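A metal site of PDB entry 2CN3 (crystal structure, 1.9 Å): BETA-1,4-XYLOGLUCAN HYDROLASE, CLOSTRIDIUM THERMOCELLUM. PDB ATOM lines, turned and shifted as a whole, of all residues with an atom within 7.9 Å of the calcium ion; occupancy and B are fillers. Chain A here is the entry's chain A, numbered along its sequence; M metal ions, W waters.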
ATOM      1  N   PRO A  26      25.874  -4.048   2.675  1.00  0.00           N
ATOM      2  CA  PRO A  26      26.848  -3.990   3.775  1.00  0.00           C
ATOM      3  C   PRO A  26      26.291  -3.677   5.172  1.00  0.00           C
ATOM      4  O   PRO A  26      26.994  -3.872   6.171  1.00  0.00           O
ATOM      5  CB  PRO A  26      27.850  -2.916   3.315  1.00  0.00           C
ATOM      6  CG  PRO A  26      27.647  -2.824   1.811  1.00  0.00           C
ATOM      7  CD  PRO A  26      26.155  -3.030   1.652  1.00  0.00           C
ATOM      8  N   GLY A  27      25.047  -3.190   5.252  1.00  0.00           N
ATOM      9  CA  GLY A  27      24.442  -2.847   6.540  1.00  0.00           C
ATOM     10  C   GLY A  27      22.926  -2.868   6.650  1.00  0.00           C
ATOM     11  O   GLY A  27      22.211  -2.563   5.695  1.00  0.00           O
ATOM     12  N   ILE A  28      22.458  -3.235   7.840  1.00  0.00           N
ATOM     13  CA  ILE A  28      21.060  -3.168   8.233  1.00  0.00           C
ATOM     14  C   ILE A  28      21.012  -2.311   9.507  1.00  0.00           C
ATOM     15  O   ILE A  28      21.868  -2.465  10.394  1.00  0.00           O
ATOM     16  CB  ILE A  28      20.492  -4.575   8.564  1.00  0.00           C
ATOM     17  CG1 ILE A  28      20.502  -5.471   7.324  1.00  0.00           C
ATOM     18  CG2 ILE A  28      19.077  -4.500   9.162  1.00  0.00           C
ATOM     19  CD1 ILE A  28      20.262  -6.948   7.630  1.00  0.00           C
ATOM     20  N   VAL A  29      20.043  -1.416   9.591  1.00  0.00           N
ATOM     21  CA  VAL A  29      19.909  -0.519  10.733  1.00  0.00           C
ATOM     22  C   VAL A  29      18.478  -0.543  11.272  1.00  0.00           C
ATOM     23  O   VAL A  29      17.533  -0.220  10.538  1.00  0.00           O
ATOM     24  CB  VAL A  29      20.334   0.930  10.380  1.00  0.00           C
ATOM     25  CG1 VAL A  29      20.179   1.864  11.592  1.00  0.00           C
ATOM     26  CG2 VAL A  29      21.776   0.963   9.898  1.00  0.00           C
ATOM     27  N   PHE A  30      18.324  -0.955  12.528  1.00  0.00           N
ATOM     28  CA  PHE A  30      17.049  -0.841  13.240  1.00  0.00           C
ATOM     29  C   PHE A  30      16.905   0.532  13.918  1.00  0.00           C
ATOM     30  O   PHE A  30      17.880   1.081  14.457  1.00  0.00           O
ATOM     31  CB  PHE A  30      16.938  -1.937  14.307  1.00  0.00           C
ATOM     32  CG  PHE A  30      16.494  -3.275  13.781  1.00  0.00           C
ATOM     33  CD1 PHE A  30      15.149  -3.654  13.826  1.00  0.00           C
ATOM     34  CD2 PHE A  30      17.418  -4.176  13.248  1.00  0.00           C
ATOM     35  CE1 PHE A  30      14.742  -4.894  13.353  1.00  0.00           C
ATOM     36  CE2 PHE A  30      17.016  -5.433  12.761  1.00  0.00           C
ATOM     37  CZ  PHE A  30      15.678  -5.792  12.814  1.00  0.00           C
ATOM     38  N   TYR A  39      15.929  -0.226   8.158  1.00  0.00           N
ATOM     39  CA  TYR A  39      16.458   0.172   6.852  1.00  0.00           C
ATOM     40  C   TYR A  39      17.642  -0.709   6.482  1.00  0.00           C
ATOM     41  O   TYR A  39      18.303  -1.288   7.354  1.00  0.00           O
ATOM     42  CB  TYR A  39      16.930   1.622   6.870  1.00  0.00           C
ATOM     43  CG  TYR A  39      15.848   2.657   7.113  1.00  0.00           C
ATOM     44  CD1 TYR A  39      15.184   3.258   6.042  1.00  0.00           C
ATOM     45  CD2 TYR A  39      15.506   3.037   8.408  1.00  0.00           C
ATOM     46  CE1 TYR A  39      14.185   4.229   6.260  1.00  0.00           C
ATOM     47  CE2 TYR A  39      14.510   4.015   8.634  1.00  0.00           C
ATOM     48  CZ  TYR A  39      13.857   4.589   7.556  1.00  0.00           C
ATOM     49  OH  TYR A  39      12.885   5.543   7.755  1.00  0.00           O
ATOM     50  N   ARG A  41      21.083  -0.864   3.612  1.00  0.00           N
ATOM     51  CA  ARG A  41      21.890  -0.145   2.621  1.00  0.00           C
ATOM     52  C   ARG A  41      22.643  -1.086   1.710  1.00  0.00           C
ATOM     53  O   ARG A  41      23.155  -2.110   2.145  1.00  0.00           O
ATOM     54  CB  ARG A  41      22.840   0.861   3.283  1.00  0.00           C
ATOM     55  CG  ARG A  41      23.888   0.260   4.233  1.00  0.00           C
ATOM     56  CD  ARG A  41      24.717   1.362   4.875  1.00  0.00           C
ATOM     57  NE  ARG A  41      25.728   0.823   5.781  1.00  0.00           N
ATOM     58  CZ  ARG A  41      26.952   0.467   5.425  1.00  0.00           C
ATOM     59  NH1 ARG A  41      27.335   0.565   4.158  1.00  0.00           N
ATOM     60  NH2 ARG A  41      27.805  -0.007   6.337  1.00  0.00           N
ATOM     61  N   ILE A  77      23.586   4.719   6.682  1.00  0.00           N
ATOM     62  CA  ILE A  77      22.200   5.132   6.846  1.00  0.00           C
ATOM     63  C   ILE A  77      21.933   5.346   8.335  1.00  0.00           C
ATOM     64  O   ILE A  77      22.368   4.555   9.179  1.00  0.00           O
ATOM     65  CB  ILE A  77      21.199   4.132   6.167  1.00  0.00           C
ATOM     66  CG1 ILE A  77      19.781   4.709   6.139  1.00  0.00           C
ATOM     67  CG2 ILE A  77      21.243   2.757   6.828  1.00  0.00           C
ATOM     68  CD1 ILE A  77      18.896   4.126   5.024  1.00  0.00           C
ATOM     69  N   SER A 132      31.355  -2.527   4.923  1.00  0.00           N
ATOM     70  CA  SER A 132      30.515  -3.052   6.013  1.00  0.00           C
ATOM     71  C   SER A 132      30.886  -2.506   7.391  1.00  0.00           C
ATOM     72  O   SER A 132      30.116  -2.635   8.340  1.00  0.00           O
ATOM     73  CB  SER A 132      30.426  -4.597   6.000  1.00  0.00           C
ATOM     74  OG  SER A 132      31.637  -5.214   6.363  1.00  0.00           O
ATOM     75  N   GLY A 134      30.943   0.319  10.070  1.00  0.00           N
ATOM     76  CA  GLY A 134      29.948   1.374  10.254  1.00  0.00           C
ATOM     77  C   GLY A 134      29.167   1.207  11.542  1.00  0.00           C
ATOM     78  O   GLY A 134      29.536   0.382  12.382  1.00  0.00           O
ATOM     79  N   GLU A 135      28.095   1.995  11.740  1.00  0.00           N
ATOM     80  CA  GLU A 135      27.669   3.038  10.807  1.00  0.00           C
ATOM     81  C   GLU A 135      28.441   4.344  10.995  1.00  0.00           C
ATOM     82  O   GLU A 135      28.608   4.837  12.128  1.00  0.00           O
ATOM     83  CB  GLU A 135      26.161   3.303  10.920  1.00  0.00           C
ATOM     84  CG  GLU A 135      25.285   2.131  10.451  1.00  0.00           C
ATOM     85  CD  GLU A 135      25.276   1.954   8.933  1.00  0.00           C
ATOM     86  OE1 GLU A 135      25.388   2.962   8.206  1.00  0.00           O
ATOM     87  OE2 GLU A 135      25.149   0.790   8.469  1.00  0.00           O
ATOM     88  N   HIS A 248      32.713  -2.453  14.159  1.00  0.00           N
ATOM     89  CA  HIS A 248      31.449  -2.112  14.775  1.00  0.00           C
ATOM     90  C   HIS A 248      31.708  -1.829  16.257  1.00  0.00           C
ATOM     91  O   HIS A 248      32.497  -2.443  16.874  1.00  0.00           O
ATOM     92  CB  HIS A 248      30.469  -3.277  14.704  1.00  0.00           C
ATOM     93  CG  HIS A 248      29.883  -3.500  13.354  1.00  0.00           C
ATOM     94  ND1 HIS A 248      29.106  -2.562  12.748  1.00  0.00           N
ATOM     95  CD2 HIS A 248      29.945  -4.537  12.511  1.00  0.00           C
ATOM     96  CE1 HIS A 248      28.776  -2.986  11.550  1.00  0.00           C
ATOM     97  NE2 HIS A 248      29.245  -4.188  11.401  1.00  0.00           N
ATOM     98  N   VAL A 250      29.068  -1.112  19.806  1.00  0.00           N
ATOM     99  CA  VAL A 250      27.732  -1.060  20.344  1.00  0.00           C
ATOM    100  C   VAL A 250      27.791  -0.841  21.837  1.00  0.00           C
ATOM    101  O   VAL A 250      28.410  -1.602  22.514  1.00  0.00           O
ATOM    102  CB  VAL A 250      26.920  -2.347  20.040  1.00  0.00           C
ATOM    103  CG1 VAL A 250      25.515  -2.276  20.625  1.00  0.00           C
ATOM    104  CG2 VAL A 250      26.894  -2.642  18.577  1.00  0.00           C
ATOM    105  N   GLY A 305      30.585  -8.657  12.158  1.00  0.00           N
ATOM    106  CA  GLY A 305      29.243  -8.388  12.655  1.00  0.00           C
ATOM    107  C   GLY A 305      29.187  -8.397  14.168  1.00  0.00           C
ATOM    108  O   GLY A 305      29.860  -9.210  14.819  1.00  0.00           O
ATOM    109  N   LEU A 306      28.426  -7.464  14.731  1.00  0.00           N
ATOM    110  CA  LEU A 306      28.212  -7.362  16.180  1.00  0.00           C
ATOM    111  C   LEU A 306      26.754  -7.007  16.445  1.00  0.00           C
ATOM    112  O   LEU A 306      26.259  -5.974  15.968  1.00  0.00           O
ATOM    113  CB  LEU A 306      29.109  -6.280  16.805  1.00  0.00           C
ATOM    114  CG  LEU A 306      28.885  -5.907  18.276  1.00  0.00           C
ATOM    115  CD1 LEU A 306      29.051  -7.111  19.215  1.00  0.00           C
ATOM    116  CD2 LEU A 306      29.825  -4.774  18.677  1.00  0.00           C
ATOM    117  N   GLY A 386      29.222  -9.012   7.288  1.00  0.00           N
ATOM    118  CA  GLY A 386      29.827  -7.843   7.954  1.00  0.00           C
ATOM    119  C   GLY A 386      28.917  -7.146   8.940  1.00  0.00           C
ATOM    120  O   GLY A 386      29.329  -6.188   9.594  1.00  0.00           O
ATOM    121  N   ASP A 387      27.681  -7.617   9.060  1.00  0.00           N
ATOM    122  CA  ASP A 387      26.682  -6.970   9.898  1.00  0.00           C
ATOM    123  C   ASP A 387      25.654  -8.009  10.322  1.00  0.00           C
ATOM    124  O   ASP A 387      25.191  -8.819   9.510  1.00  0.00           O
ATOM    125  CB  ASP A 387      26.011  -5.819   9.137  1.00  0.00           C
ATOM    126  CG  ASP A 387      25.269  -4.851  10.035  1.00  0.00           C
ATOM    127  OD1 ASP A 387      25.833  -4.379  11.047  1.00  0.00           O
ATOM    128  OD2 ASP A 387      24.101  -4.519   9.721  1.00  0.00           O
ATOM    129  N   ILE A 388      25.311  -7.979  11.600  1.00  0.00           N
ATOM    130  CA  ILE A 388      24.274  -8.835  12.166  1.00  0.00           C
ATOM    131  C   ILE A 388      23.499  -7.964  13.160  1.00  0.00           C
ATOM    132  O   ILE A 388      24.082  -7.115  13.844  1.00  0.00           O
ATOM    133  CB  ILE A 388      24.870 -10.136  12.794  1.00  0.00           C
ATOM    134  CG1 ILE A 388      23.746 -11.084  13.277  1.00  0.00           C
ATOM    135  CG2 ILE A 388      25.906  -9.820  13.894  1.00  0.00           C
ATOM    136  CD1 ILE A 388      24.236 -12.522  13.580  1.00  0.00           C
ATOM    137  N   GLU A 389      22.183  -8.164  13.215  1.00  0.00           N
ATOM    138  CA  GLU A 389      21.330  -7.364  14.091  1.00  0.00           C
ATOM    139  C   GLU A 389      20.369  -8.250  14.867  1.00  0.00           C
ATOM    140  O   GLU A 389      19.796  -9.191  14.317  1.00  0.00           O
ATOM    141  CB  GLU A 389      20.533  -6.343  13.280  1.00  0.00           C
ATOM    142  CG  GLU A 389      21.379  -5.312  12.535  1.00  0.00           C
ATOM    143  CD  GLU A 389      21.981  -4.280  13.462  1.00  0.00           C
ATOM    144  OE1 GLU A 389      21.318  -3.904  14.450  1.00  0.00           O
ATOM    145  OE2 GLU A 389      23.111  -3.822  13.194  1.00  0.00           O
ATOM    146  N   MET A 399      18.595 -10.586  12.016  1.00  0.00           N
ATOM    147  CA  MET A 399      18.863 -10.474  10.580  1.00  0.00           C
ATOM    148  C   MET A 399      20.374 -10.318  10.393  1.00  0.00           C
ATOM    149  O   MET A 399      21.033  -9.664  11.199  1.00  0.00           O
ATOM    150  CB  MET A 399      18.180  -9.253   9.967  1.00  0.00           C
ATOM    151  CG  MET A 399      16.664  -9.364   9.758  1.00  0.00           C
ATOM    152  SD  MET A 399      16.006  -7.901   8.894  1.00  0.00           S
ATOM    153  CE  MET A 399      14.268  -8.360   8.776  1.00  0.00           C
ATOM    154  N   VAL A 401      23.536  -9.999   6.996  1.00  0.00           N
ATOM    155  CA  VAL A 401      23.801  -9.787   5.567  1.00  0.00           C
ATOM    156  C   VAL A 401      24.780 -10.817   5.050  1.00  0.00           C
ATOM    157  O   VAL A 401      25.576 -11.371   5.816  1.00  0.00           O
ATOM    158  CB  VAL A 401      24.348  -8.350   5.270  1.00  0.00           C
ATOM    159  CG1 VAL A 401      23.426  -7.277   5.869  1.00  0.00           C
ATOM    160  CG2 VAL A 401      25.774  -8.183   5.787  1.00  0.00           C
HETATM  161 CA    CA M   1      24.092  -2.667  11.403  1.00  0.00          CA
HETATM  162  O   HOH W   1      25.868  -1.917  12.942  1.00  0.00           O
HETATM  163  O   HOH W   2      25.270  -1.371   9.849  1.00  0.00           O
HETATM  164  O   HOH W   3      23.227  -0.654  12.700  1.00  0.00           O
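The backbone NH of Glu 389 sits at hydrogen-bond distance from the backbone carbonyl oxygen of Met 399.
The side-chain carboxylate (OD1) of Asp 387 sits close to a ring nitrogen (NE2) of His 248 (3.4 Å).
The backbone carbonyl oxygen of Asp 387 sits at hydrogen-bond distance from the backbone NH of Val 401, at 3.2 Å.
Of the 21 residues printed, 3 come within 4 Å of the calcium ion.
The nearest printed residue that does not touch the calcium ion is Val 29 (4.6 Å).
The calcium ion is bound by water W2 (2.3 Å), the side-chain carboxylate (OE2) of Glu 389 (2.3 Å), the backbone carbonyl oxygen (O) of Ile 28 (2.5 Å), water W1 (2.5 Å), the side-chain carboxylate (OD1) of Asp 387 (2.5 Å), the side-chain carboxylate (OD2) of Asp 387 (2.5 Å) and water W3 (2.5 Å).
The calcium ion has seven donor atoms within binding distance.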
